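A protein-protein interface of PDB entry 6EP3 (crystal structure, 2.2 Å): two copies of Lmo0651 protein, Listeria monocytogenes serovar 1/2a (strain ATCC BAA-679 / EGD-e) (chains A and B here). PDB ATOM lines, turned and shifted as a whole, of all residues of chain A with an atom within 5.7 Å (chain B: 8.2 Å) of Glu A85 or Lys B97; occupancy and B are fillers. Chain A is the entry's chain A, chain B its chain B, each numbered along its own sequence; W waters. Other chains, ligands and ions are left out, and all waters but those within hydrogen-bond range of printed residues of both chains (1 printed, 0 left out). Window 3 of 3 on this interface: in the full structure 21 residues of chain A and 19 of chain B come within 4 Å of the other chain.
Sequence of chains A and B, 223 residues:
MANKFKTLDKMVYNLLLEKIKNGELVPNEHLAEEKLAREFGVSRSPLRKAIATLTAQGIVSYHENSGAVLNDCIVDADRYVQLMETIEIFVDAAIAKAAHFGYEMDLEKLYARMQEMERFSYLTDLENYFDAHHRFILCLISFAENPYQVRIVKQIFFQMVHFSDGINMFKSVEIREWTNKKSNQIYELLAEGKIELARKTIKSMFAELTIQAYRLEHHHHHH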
ATOM      1  N   TYR A  80      -2.416  15.796 -13.248  1.00  0.00           N
ATOM      2  CA  TYR A  80      -1.277  15.652 -14.147  1.00  0.00           C
ATOM      3  C   TYR A  80      -1.579  14.634 -15.238  1.00  0.00           C
ATOM      4  O   TYR A  80      -1.300  14.873 -16.418  1.00  0.00           O
ATOM      5  CB  TYR A  80      -0.038  15.246 -13.352  1.00  0.00           C
ATOM      6  CG  TYR A  80       1.273  15.462 -14.075  1.00  0.00           C
ATOM      7  CD1 TYR A  80       1.910  16.696 -14.042  1.00  0.00           C
ATOM      8  CD2 TYR A  80       1.882  14.429 -14.777  1.00  0.00           C
ATOM      9  CE1 TYR A  80       3.109  16.898 -14.693  1.00  0.00           C
ATOM     10  CE2 TYR A  80       3.085  14.622 -15.431  1.00  0.00           C
ATOM     11  CZ  TYR A  80       3.694  15.859 -15.387  1.00  0.00           C
ATOM     12  OH  TYR A  80       4.891  16.060 -16.036  1.00  0.00           O
ATOM     13  N   VAL A  81      -2.181  13.504 -14.861  1.00  0.00           N
ATOM     14  CA  VAL A  81      -2.508  12.470 -15.837  1.00  0.00           C
ATOM     15  C   VAL A  81      -3.594  12.954 -16.792  1.00  0.00           C
ATOM     16  O   VAL A  81      -3.580  12.623 -17.981  1.00  0.00           O
ATOM     17  CB  VAL A  81      -2.911  11.172 -15.114  1.00  0.00           C
ATOM     18  CG1 VAL A  81      -3.419  10.138 -16.102  1.00  0.00           C
ATOM     19  CG2 VAL A  81      -1.725  10.623 -14.337  1.00  0.00           C
ATOM     20  N   GLN A  82      -4.539  13.756 -16.300  1.00  0.00           N
ATOM     21  CA  GLN A  82      -5.563  14.317 -17.183  1.00  0.00           C
ATOM     22  C   GLN A  82      -4.943  15.232 -18.237  1.00  0.00           C
ATOM     23  O   GLN A  82      -5.257  15.137 -19.437  1.00  0.00           O
ATOM     24  CB  GLN A  82      -6.604  15.071 -16.358  1.00  0.00           C
ATOM     25  CG  GLN A  82      -7.557  14.177 -15.574  1.00  0.00           C
ATOM     26  CD  GLN A  82      -8.530  14.965 -14.707  1.00  0.00           C
ATOM     27  OE1 GLN A  82      -8.258  16.097 -14.308  1.00  0.00           O
ATOM     28  NE2 GLN A  82      -9.680  14.368 -14.428  1.00  0.00           N
ATOM     29  N   LEU A  83      -4.058  16.133 -17.799  1.00  0.00           N
ATOM     30  CA  LEU A  83      -3.323  16.981 -18.736  1.00  0.00           C
ATOM     31  C   LEU A  83      -2.512  16.155 -19.724  1.00  0.00           C
ATOM     32  O   LEU A  83      -2.466  16.472 -20.919  1.00  0.00           O
ATOM     33  CB  LEU A  83      -2.412  17.944 -17.977  1.00  0.00           C
ATOM     34  CG  LEU A  83      -3.155  18.900 -17.043  1.00  0.00           C
ATOM     35  CD1 LEU A  83      -2.193  19.734 -16.224  1.00  0.00           C
ATOM     36  CD2 LEU A  83      -4.087  19.789 -17.856  1.00  0.00           C
ATOM     37  N   MET A  84      -1.866  15.089 -19.251  1.00  0.00           N
ATOM     38  CA  MET A  84      -1.048  14.288 -20.155  1.00  0.00           C
ATOM     39  C   MET A  84      -1.902  13.516 -21.151  1.00  0.00           C
ATOM     40  O   MET A  84      -1.481  13.308 -22.293  1.00  0.00           O
ATOM     41  CB  MET A  84      -0.148  13.346 -19.362  1.00  0.00           C
ATOM     42  CG  MET A  84       1.272  13.870 -19.224  1.00  0.00           C
ATOM     43  SD  MET A  84       2.438  12.571 -18.808  1.00  0.00           S
ATOM     44  CE  MET A  84       1.600  11.834 -17.407  1.00  0.00           C
ATOM     45  N   GLU A  85      -3.101  13.099 -20.750  1.00  0.00           N
ATOM     46  CA  GLU A  85      -4.012  12.477 -21.704  1.00  0.00           C
ATOM     47  C   GLU A  85      -4.412  13.466 -22.790  1.00  0.00           C
ATOM     48  O   GLU A  85      -4.461  13.114 -23.976  1.00  0.00           O
ATOM     49  CB  GLU A  85      -5.245  11.937 -20.981  1.00  0.00           C
ATOM     50  CG  GLU A  85      -4.944  10.785 -20.034  1.00  0.00           C
ATOM     51  CD  GLU A  85      -6.143  10.373 -19.200  1.00  0.00           C
ATOM     52  OE1 GLU A  85      -6.091   9.287 -18.588  1.00  0.00           O
ATOM     53  OE2 GLU A  85      -7.133  11.133 -19.148  1.00  0.00           O
ATOM     54  N   THR A  86      -4.683  14.717 -22.408  1.00  0.00           N
ATOM     55  CA  THR A  86      -4.952  15.740 -23.420  1.00  0.00           C
ATOM     56  C   THR A  86      -3.761  15.913 -24.364  1.00  0.00           C
ATOM     57  O   THR A  86      -3.917  15.931 -25.598  1.00  0.00           O
ATOM     58  CB  THR A  86      -5.308  17.061 -22.739  1.00  0.00           C
ATOM     59  OG1 THR A  86      -6.484  16.881 -21.938  1.00  0.00           O
ATOM     60  CG2 THR A  86      -5.563  18.148 -23.771  1.00  0.00           C
ATOM     61  N   ILE A  87      -2.559  16.036 -23.795  1.00  0.00           N
ATOM     62  CA  ILE A  87      -1.358  16.207 -24.609  1.00  0.00           C
ATOM     63  C   ILE A  87      -1.211  15.056 -25.591  1.00  0.00           C
ATOM     64  O   ILE A  87      -0.943  15.264 -26.781  1.00  0.00           O
ATOM     65  CB  ILE A  87      -0.112  16.330 -23.712  1.00  0.00           C
ATOM     66  CG1 ILE A  87      -0.165  17.611 -22.885  1.00  0.00           C
ATOM     67  CG2 ILE A  87       1.162  16.302 -24.551  1.00  0.00           C
ATOM     68  CD1 ILE A  87       0.875  17.650 -21.801  1.00  0.00           C
ATOM     69  N   GLU A  88      -1.421  13.829 -25.124  1.00  0.00           N
ATOM     70  CA  GLU A  88      -1.162  12.686 -25.984  1.00  0.00           C
ATOM     71  C   GLU A  88      -2.249  12.532 -27.037  1.00  0.00           C
ATOM     72  O   GLU A  88      -1.960  12.074 -28.145  1.00  0.00           O
ATOM     73  CB  GLU A  88      -0.988  11.418 -25.143  1.00  0.00           C
ATOM     74  CG  GLU A  88      -2.187  10.535 -24.993  1.00  0.00           C
ATOM     75  CD  GLU A  88      -1.793   9.115 -24.628  1.00  0.00           C
ATOM     76  OE1 GLU A  88      -1.916   8.747 -23.441  1.00  0.00           O
ATOM     77  OE2 GLU A  88      -1.345   8.370 -25.524  1.00  0.00           O
ATOM     78  N   ILE A  89      -3.486  12.932 -26.729  1.00  0.00           N
ATOM     79  CA  ILE A  89      -4.518  12.994 -27.762  1.00  0.00           C
ATOM     80  C   ILE A  89      -4.074  13.927 -28.883  1.00  0.00           C
ATOM     81  O   ILE A  89      -4.145  13.587 -30.074  1.00  0.00           O
ATOM     82  CB  ILE A  89      -5.858  13.446 -27.147  1.00  0.00           C
ATOM     83  CG1 ILE A  89      -6.494  12.317 -26.337  1.00  0.00           C
ATOM     84  CG2 ILE A  89      -6.816  13.955 -28.216  1.00  0.00           C
ATOM     85  CD1 ILE A  89      -7.455  12.820 -25.271  1.00  0.00           C
ATOM     86  N   PHE A  90      -3.558  15.102 -28.509  1.00  0.00           N
ATOM     87  CA  PHE A  90      -3.067  16.042 -29.517  1.00  0.00           C
ATOM     88  C   PHE A  90      -1.918  15.445 -30.329  1.00  0.00           C
ATOM     89  O   PHE A  90      -1.894  15.557 -31.559  1.00  0.00           O
ATOM     90  CB  PHE A  90      -2.626  17.341 -28.846  1.00  0.00           C
ATOM     91  CG  PHE A  90      -3.741  18.311 -28.629  1.00  0.00           C
ATOM     92  CD1 PHE A  90      -4.627  18.609 -29.646  1.00  0.00           C
ATOM     93  CD2 PHE A  90      -3.926  18.901 -27.390  1.00  0.00           C
ATOM     94  CE1 PHE A  90      -5.666  19.495 -29.438  1.00  0.00           C
ATOM     95  CE2 PHE A  90      -4.961  19.790 -27.175  1.00  0.00           C
ATOM     96  CZ  PHE A  90      -5.834  20.088 -28.199  1.00  0.00           C
ATOM     97  N   PHE B  90     -11.238  15.801 -29.436  1.00  0.00           N
ATOM     98  CA  PHE B  90     -11.680  15.771 -28.041  1.00  0.00           C
ATOM     99  C   PHE B  90     -12.940  14.919 -27.860  1.00  0.00           C
ATOM    100  O   PHE B  90     -13.023  14.111 -26.926  1.00  0.00           O
ATOM    101  CB  PHE B  90     -11.918  17.192 -27.534  1.00  0.00           C
ATOM    102  CG  PHE B  90     -10.680  17.858 -27.014  1.00  0.00           C
ATOM    103  CD1 PHE B  90      -9.827  17.186 -26.154  1.00  0.00           C
ATOM    104  CD2 PHE B  90     -10.366  19.153 -27.385  1.00  0.00           C
ATOM    105  CE1 PHE B  90      -8.682  17.794 -25.677  1.00  0.00           C
ATOM    106  CE2 PHE B  90      -9.225  19.768 -26.909  1.00  0.00           C
ATOM    107  CZ  PHE B  90      -8.381  19.088 -26.054  1.00  0.00           C
ATOM    108  N   VAL B  91     -13.925  15.078 -28.746  1.00  0.00           N
ATOM    109  CA  VAL B  91     -15.188  14.345 -28.606  1.00  0.00           C
ATOM    110  C   VAL B  91     -14.957  12.846 -28.767  1.00  0.00           C
ATOM    111  O   VAL B  91     -15.446  12.026 -27.970  1.00  0.00           O
ATOM    112  CB  VAL B  91     -16.228  14.858 -29.620  1.00  0.00           C
ATOM    113  CG1 VAL B  91     -17.485  14.000 -29.578  1.00  0.00           C
ATOM    114  CG2 VAL B  91     -16.569  16.315 -29.363  1.00  0.00           C
ATOM    115  N   ASP B  92     -14.227  12.462 -29.817  1.00  0.00           N
ATOM    116  CA  ASP B  92     -13.990  11.048 -30.072  1.00  0.00           C
ATOM    117  C   ASP B  92     -13.207  10.407 -28.936  1.00  0.00           C
ATOM    118  O   ASP B  92     -13.536   9.297 -28.500  1.00  0.00           O
ATOM    119  CB  ASP B  92     -13.259  10.868 -31.402  1.00  0.00           C
ATOM    120  CG  ASP B  92     -13.063   9.409 -31.760  1.00  0.00           C
ATOM    121  OD1 ASP B  92     -14.060   8.749 -32.125  1.00  0.00           O
ATOM    122  OD2 ASP B  92     -11.916   8.921 -31.671  1.00  0.00           O
ATOM    123  N   ALA B  93     -12.168  11.087 -28.436  1.00  0.00           N
ATOM    124  CA  ALA B  93     -11.409  10.531 -27.322  1.00  0.00           C
ATOM    125  C   ALA B  93     -12.258  10.447 -26.059  1.00  0.00           C
ATOM    126  O   ALA B  93     -12.111   9.508 -25.272  1.00  0.00           O
ATOM    127  CB  ALA B  93     -10.148  11.354 -27.071  1.00  0.00           C
ATOM    128  N   ALA B  94     -13.152  11.415 -25.847  1.00  0.00           N
ATOM    129  CA  ALA B  94     -14.047  11.347 -24.698  1.00  0.00           C
ATOM    130  C   ALA B  94     -14.909  10.097 -24.761  1.00  0.00           C
ATOM    131  O   ALA B  94     -15.020   9.350 -23.778  1.00  0.00           O
ATOM    132  CB  ALA B  94     -14.926  12.597 -24.637  1.00  0.00           C
ATOM    133  N   ILE B  95     -15.525   9.851 -25.918  1.00  0.00           N
ATOM    134  CA  ILE B  95     -16.390   8.682 -26.048  1.00  0.00           C
ATOM    135  C   ILE B  95     -15.578   7.400 -25.902  1.00  0.00           C
ATOM    136  O   ILE B  95     -16.006   6.446 -25.238  1.00  0.00           O
ATOM    137  CB  ILE B  95     -17.169   8.733 -27.375  1.00  0.00           C
ATOM    138  CG1 ILE B  95     -18.042   9.987 -27.418  1.00  0.00           C
ATOM    139  CG2 ILE B  95     -18.063   7.522 -27.522  1.00  0.00           C
ATOM    140  CD1 ILE B  95     -18.852  10.191 -26.157  1.00  0.00           C
ATOM    141  N   ALA B  96     -14.380   7.367 -26.489  1.00  0.00           N
ATOM    142  CA  ALA B  96     -13.539   6.179 -26.389  1.00  0.00           C
ATOM    143  C   ALA B  96     -13.151   5.897 -24.941  1.00  0.00           C
ATOM    144  O   ALA B  96     -13.204   4.751 -24.484  1.00  0.00           O
ATOM    145  CB  ALA B  96     -12.292   6.346 -27.262  1.00  0.00           C
ATOM    146  N   LYS B  97     -12.745   6.934 -24.207  1.00  0.00           N
ATOM    147  CA  LYS B  97     -12.358   6.746 -22.814  1.00  0.00           C
ATOM    148  C   LYS B  97     -13.538   6.289 -21.972  1.00  0.00           C
ATOM    149  O   LYS B  97     -13.412   5.356 -21.168  1.00  0.00           O
ATOM    150  CB  LYS B  97     -11.766   8.040 -22.255  1.00  0.00           C
ATOM    151  CG  LYS B  97     -11.212   7.908 -20.842  1.00  0.00           C
ATOM    152  CD  LYS B  97     -10.800   9.261 -20.279  1.00  0.00           C
ATOM    153  CE  LYS B  97     -10.304   9.143 -18.843  1.00  0.00           C
ATOM    154  NZ  LYS B  97     -10.099  10.482 -18.227  1.00  0.00           N
ATOM    155  N   ALA B  98     -14.699   6.929 -22.144  1.00  0.00           N
ATOM    156  CA  ALA B  98     -15.868   6.538 -21.364  1.00  0.00           C
ATOM    157  C   ALA B  98     -16.247   5.089 -21.634  1.00  0.00           C
ATOM    158  O   ALA B  98     -16.530   4.330 -20.700  1.00  0.00           O
ATOM    159  CB  ALA B  98     -17.043   7.467 -21.670  1.00  0.00           C
ATOM    160  N   ALA B  99     -16.218   4.677 -22.903  1.00  0.00           N
ATOM    161  CA  ALA B  99     -16.571   3.303 -23.231  1.00  0.00           C
ATOM    162  C   ALA B  99     -15.528   2.318 -22.720  1.00  0.00           C
ATOM    163  O   ALA B  99     -15.873   1.213 -22.283  1.00  0.00           O
ATOM    164  CB  ALA B  99     -16.752   3.158 -24.739  1.00  0.00           C
ATOM    165  N   HIS B 100     -14.249   2.695 -22.756  1.00  0.00           N
ATOM    166  CA  HIS B 100     -13.204   1.751 -22.381  1.00  0.00           C
ATOM    167  C   HIS B 100     -13.138   1.555 -20.873  1.00  0.00           C
ATOM    168  O   HIS B 100     -12.976   0.425 -20.400  1.00  0.00           O
ATOM    169  CB  HIS B 100     -11.852   2.225 -22.919  1.00  0.00           C
ATOM    170  CG  HIS B 100     -10.711   1.333 -22.547  1.00  0.00           C
ATOM    171  ND1 HIS B 100     -10.413   0.177 -23.238  1.00  0.00           N
ATOM    172  CD2 HIS B 100      -9.792   1.424 -21.556  1.00  0.00           C
ATOM    173  CE1 HIS B 100      -9.362  -0.404 -22.689  1.00  0.00           C
ATOM    174  NE2 HIS B 100      -8.966   0.332 -21.666  1.00  0.00           N
ATOM    175  N   PHE B 101     -13.280   2.631 -20.103  1.00  0.00           N
ATOM    176  CA  PHE B 101     -13.212   2.539 -18.651  1.00  0.00           C
ATOM    177  C   PHE B 101     -14.573   2.312 -18.006  1.00  0.00           C
ATOM    178  O   PHE B 101     -14.653   2.227 -16.776  1.00  0.00           O
ATOM    179  CB  PHE B 101     -12.568   3.801 -18.071  1.00  0.00           C
ATOM    180  CG  PHE B 101     -11.093   3.910 -18.345  1.00  0.00           C
ATOM    181  CD1 PHE B 101     -10.503   5.146 -18.554  1.00  0.00           C
ATOM    182  CD2 PHE B 101     -10.299   2.777 -18.399  1.00  0.00           C
ATOM    183  CE1 PHE B 101      -9.146   5.249 -18.807  1.00  0.00           C
ATOM    184  CE2 PHE B 101      -8.941   2.874 -18.652  1.00  0.00           C
ATOM    185  CZ  PHE B 101      -8.366   4.110 -18.856  1.00  0.00           C
ATOM    186  N   GLY B 102     -15.634   2.206 -18.798  1.00  0.00           N
ATOM    187  CA  GLY B 102     -16.950   1.919 -18.250  1.00  0.00           C
ATOM    188  C   GLY B 102     -17.493   3.013 -17.360  1.00  0.00           C
ATOM    189  O   GLY B 102     -18.205   2.723 -16.389  1.00  0.00           O
ATOM    190  N   TYR B 103     -17.195   4.269 -17.679  1.00  0.00           N
ATOM    191  CA  TYR B 103     -17.781   5.368 -16.929  1.00  0.00           C
ATOM    192  C   TYR B 103     -19.293   5.413 -17.138  1.00  0.00           C
ATOM    193  O   TYR B 103     -19.842   4.829 -18.076  1.00  0.00           O
ATOM    194  CB  TYR B 103     -17.154   6.702 -17.337  1.00  0.00           C
ATOM    195  CG  TYR B 103     -15.677   6.800 -17.049  1.00  0.00           C
ATOM    196  CD1 TYR B 103     -14.848   7.605 -17.823  1.00  0.00           C
ATOM    197  CD2 TYR B 103     -15.110   6.095 -15.997  1.00  0.00           C
ATOM    198  CE1 TYR B 103     -13.500   7.704 -17.556  1.00  0.00           C
ATOM    199  CE2 TYR B 103     -13.763   6.185 -15.722  1.00  0.00           C
ATOM    200  CZ  TYR B 103     -12.959   6.990 -16.504  1.00  0.00           C
ATOM    201  OH  TYR B 103     -11.612   7.079 -16.232  1.00  0.00           O
ATOM    202  N   MET B 105     -22.102   7.651 -18.276  1.00  0.00           N
ATOM    203  CA  MET B 105     -22.379   8.865 -19.030  1.00  0.00           C
ATOM    204  C   MET B 105     -23.715   9.458 -18.602  1.00  0.00           C
ATOM    205  O   MET B 105     -24.727   8.753 -18.544  1.00  0.00           O
ATOM    206  CB  MET B 105     -22.392   8.568 -20.528  1.00  0.00           C
ATOM    207  CG  MET B 105     -21.127   7.912 -21.046  1.00  0.00           C
ATOM    208  SD  MET B 105     -21.300   7.428 -22.772  1.00  0.00           S
ATOM    209  CE  MET B 105     -21.074   5.657 -22.653  1.00  0.00           C
ATOM    210  N   ILE B 141     -18.124  15.864 -24.525  1.00  0.00           N
ATOM    211  CA  ILE B 141     -16.724  15.934 -24.107  1.00  0.00           C
ATOM    212  C   ILE B 141     -16.593  15.705 -22.607  1.00  0.00           C
ATOM    213  O   ILE B 141     -15.646  15.057 -22.142  1.00  0.00           O
ATOM    214  CB  ILE B 141     -16.106  17.275 -24.534  1.00  0.00           C
ATOM    215  CG1 ILE B 141     -16.104  17.373 -26.055  1.00  0.00           C
ATOM    216  CG2 ILE B 141     -14.691  17.415 -23.981  1.00  0.00           C
ATOM    217  CD1 ILE B 141     -15.427  18.592 -26.582  1.00  0.00           C
ATOM    218  N   SER B 142     -17.539  16.227 -21.827  1.00  0.00           N
ATOM    219  CA  SER B 142     -17.529  16.027 -20.387  1.00  0.00           C
ATOM    220  C   SER B 142     -17.677  14.564 -20.030  1.00  0.00           C
ATOM    221  O   SER B 142     -17.310  14.164 -18.921  1.00  0.00           O
ATOM    222  CB  SER B 142     -18.658  16.823 -19.735  1.00  0.00           C
ATOM    223  OG  SER B 142     -19.865  16.075 -19.747  1.00  0.00           O
ATOM    224  N   PHE B 143     -18.211  13.758 -20.949  1.00  0.00           N
ATOM    225  CA  PHE B 143     -18.231  12.320 -20.695  1.00  0.00           C
ATOM    226  C   PHE B 143     -16.840  11.757 -20.401  1.00  0.00           C
ATOM    227  O   PHE B 143     -16.736  10.677 -19.811  1.00  0.00           O
ATOM    228  CB  PHE B 143     -18.862  11.578 -21.875  1.00  0.00           C
ATOM    229  CG  PHE B 143     -20.355  11.763 -21.978  1.00  0.00           C
ATOM    230  CD1 PHE B 143     -21.068  12.348 -20.944  1.00  0.00           C
ATOM    231  CD2 PHE B 143     -21.041  11.345 -23.107  1.00  0.00           C
ATOM    232  CE1 PHE B 143     -22.441  12.516 -21.034  1.00  0.00           C
ATOM    233  CE2 PHE B 143     -22.407  11.508 -23.204  1.00  0.00           C
ATOM    234  CZ  PHE B 143     -23.110  12.097 -22.163  1.00  0.00           C
ATOM    235  N   ALA B 144     -15.770  12.459 -20.783  1.00  0.00           N
ATOM    236  CA  ALA B 144     -14.425  12.017 -20.435  1.00  0.00           C
ATOM    237  C   ALA B 144     -14.043  12.340 -18.997  1.00  0.00           C
ATOM    238  O   ALA B 144     -13.021  11.834 -18.523  1.00  0.00           O
ATOM    239  CB  ALA B 144     -13.387  12.640 -21.375  1.00  0.00           C
ATOM    240  N   GLU B 145     -14.828  13.166 -18.300  1.00  0.00           N
ATOM    241  CA  GLU B 145     -14.483  13.632 -16.957  1.00  0.00           C
ATOM    242  C   GLU B 145     -13.123  14.327 -16.952  1.00  0.00           C
ATOM    243  O   GLU B 145     -12.216  13.980 -16.195  1.00  0.00           O
ATOM    244  CB  GLU B 145     -14.550  12.503 -15.925  1.00  0.00           C
ATOM    245  CG  GLU B 145     -15.979  12.046 -15.647  1.00  0.00           C
ATOM    246  CD  GLU B 145     -16.130  10.545 -15.561  1.00  0.00           C
ATOM    247  OE1 GLU B 145     -16.318   9.916 -16.620  1.00  0.00           O
ATOM    248  OE2 GLU B 145     -16.068  10.000 -14.438  1.00  0.00           O
ATOM    249  N   ASN B 146     -12.994  15.326 -17.826  1.00  0.00           N
ATOM    250  CA  ASN B 146     -11.761  16.094 -17.971  1.00  0.00           C
ATOM    251  C   ASN B 146     -12.143  17.566 -18.081  1.00  0.00           C
ATOM    252  O   ASN B 146     -12.350  18.108 -19.181  1.00  0.00           O
ATOM    253  CB  ASN B 146     -10.955  15.629 -19.183  1.00  0.00           C
ATOM    254  CG  ASN B 146      -9.485  15.921 -19.039  1.00  0.00           C
ATOM    255  OD1 ASN B 146      -9.100  16.942 -18.472  1.00  0.00           O
ATOM    256  ND2 ASN B 146      -8.650  15.026 -19.556  1.00  0.00           N
ATOM    257  N   PRO B 147     -12.241  18.249 -16.937  1.00  0.00           N
ATOM    258  CA  PRO B 147     -12.630  19.666 -16.957  1.00  0.00           C
ATOM    259  C   PRO B 147     -11.662  20.541 -17.729  1.00  0.00           C
ATOM    260  O   PRO B 147     -12.079  21.572 -18.271  1.00  0.00           O
ATOM    261  CB  PRO B 147     -12.664  20.038 -15.468  1.00  0.00           C
ATOM    262  CG  PRO B 147     -12.844  18.729 -14.748  1.00  0.00           C
ATOM    263  CD  PRO B 147     -12.106  17.720 -15.570  1.00  0.00           C
ATOM    264  N   GLN B 149     -10.293  19.755 -20.564  1.00  0.00           N
ATOM    265  CA  GLN B 149     -10.763  19.662 -21.940  1.00  0.00           C
ATOM    266  C   GLN B 149     -12.053  20.440 -22.127  1.00  0.00           C
ATOM    267  O   GLN B 149     -12.251  21.086 -23.167  1.00  0.00           O
ATOM    268  CB  GLN B 149     -10.953  18.200 -22.334  1.00  0.00           C
ATOM    269  CG  GLN B 149      -9.689  17.356 -22.213  1.00  0.00           C
ATOM    270  CD  GLN B 149      -9.922  15.909 -22.601  1.00  0.00           C
ATOM    271  OE1 GLN B 149     -11.066  15.468 -22.732  1.00  0.00           O
ATOM    272  NE2 GLN B 149      -8.837  15.163 -22.803  1.00  0.00           N
ATOM    273  N   ILE B 195     -21.134   1.879 -29.360  1.00  0.00           N
ATOM    274  CA  ILE B 195     -20.152   2.943 -29.198  1.00  0.00           C
ATOM    275  C   ILE B 195     -19.480   3.268 -30.524  1.00  0.00           C
ATOM    276  O   ILE B 195     -19.307   4.440 -30.874  1.00  0.00           O
ATOM    277  CB  ILE B 195     -19.121   2.556 -28.129  1.00  0.00           C
ATOM    278  CG1 ILE B 195     -19.836   2.168 -26.835  1.00  0.00           C
ATOM    279  CG2 ILE B 195     -18.172   3.711 -27.895  1.00  0.00           C
ATOM    280  CD1 ILE B 195     -20.711   3.262 -26.283  1.00  0.00           C
ATOM    281  N   ARG B 199     -19.526   6.777 -32.534  1.00  0.00           N
ATOM    282  CA  ARG B 199     -18.323   7.507 -32.915  1.00  0.00           C
ATOM    283  C   ARG B 199     -18.309   7.803 -34.409  1.00  0.00           C
ATOM    284  O   ARG B 199     -17.940   8.907 -34.830  1.00  0.00           O
ATOM    285  CB  ARG B 199     -17.081   6.723 -32.504  1.00  0.00           C
ATOM    286  CG  ARG B 199     -16.931   6.571 -31.006  1.00  0.00           C
ATOM    287  CD  ARG B 199     -15.796   5.627 -30.674  1.00  0.00           C
ATOM    288  NE  ARG B 199     -14.501   6.250 -30.906  1.00  0.00           N
ATOM    289  CZ  ARG B 199     -13.341   5.619 -30.771  1.00  0.00           C
ATOM    290  NH1 ARG B 199     -13.321   4.344 -30.409  1.00  0.00           N
ATOM    291  NH2 ARG B 199     -12.205   6.261 -30.997  1.00  0.00           N
HETATM  292  O   HOH W   1      -9.036  12.422 -20.181  1.00  0.00           O
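Of the 25 printed residues of chain B, 6 touch a printed residue of chain A.
Printed residues of chain B that touch a printed residue of chain A: Phe B90, Ala B93, Lys B97, Glu B145, Asn B146 and Gln B149.
Hydrophobic or aromatic side chains of chain B within 4 Å of the printed part of chain A: Phe B90 and Ala B93.
Of the 11 printed residues of chain A, 5 touch a printed residue of chain B.
Among the printed residues, 9 pairs touch across the chains.
Among the printed residues, Asp or Glu carboxylates within 4 Å of a Lys or Arg side-chain nitrogen of the other chain: Glu A85 with Lys B97 (3.2 Å).
OG1 of Thr A86 is in hydrogen-bond range of O of Gln A82 (3.3 Å).
The side-chain amino group (NZ) of Lys B97 sits at hydrogen-bond distance from the backbone carbonyl oxygen (O) of Ala B144 (3.2 Å).
NE2 of Gln B149 sits close to ND2 of Asn B146 (3.3 Å).
Water W1 lies within hydrogen-bond range of the side-chain carboxylate of Glu A85 (2.5 Å), the side-chain amide nitrogen of Asn B146 (2.7 Å) and the side-chain amino group of Lys B97 (3.0 Å).
Phe A90 touches its own counterpart, Phe B90.
Position printed for both chains: 90.
Of the 9 pairs that touch across the chains among the printed residues, 1 has its exchanged pair printed and touching as well.
NE2 of Gln A82 sits at hydrogen-bond distance from O of Glu B145, 3.1 Å away.
O of Gln A82 lies within hydrogen-bond range of ND2 of Asn B146, at 3.4 Å.
OE2 of Glu A85 lies within salt-bridge range of NZ of Lys B97.
OG1 of Thr A86 lies within hydrogen-bond range of NE2 of Gln B149, at 3.0 Å.
Of chain B, only Lys B97 comes within 4 Å of Glu A85.
Lys B97 touches just one residue of chain A: Glu A85 (3.2 Å).
Printed residues of chain A within 4 Å of Asn B146: Gln A82 and Thr A86.
Of the printed residues of chain A, Phe B90 touches Thr A86 (3.7 Å) and Phe A90 (3.5 Å).
Ala B94 touches none of the printed residues of chain A.
The nearest residue of chain A that does not touch Lys B97 is Gln A82 (5.2 Å).
The nearest printed residue of chain A that does not touch Ala B93 is Glu A85 (6.7 Å).
Among the printed residues, pairs that only touch across the chains: Thr A86 with Phe B90 (3.7 Å), Thr A86 with Asn B146 (3.7 Å), Ile A89 with Ala B93 (3.6 Å), Ile A89 with Gln B149 (3.7 Å) and Phe A90 with Phe B90 (3.5 Å).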
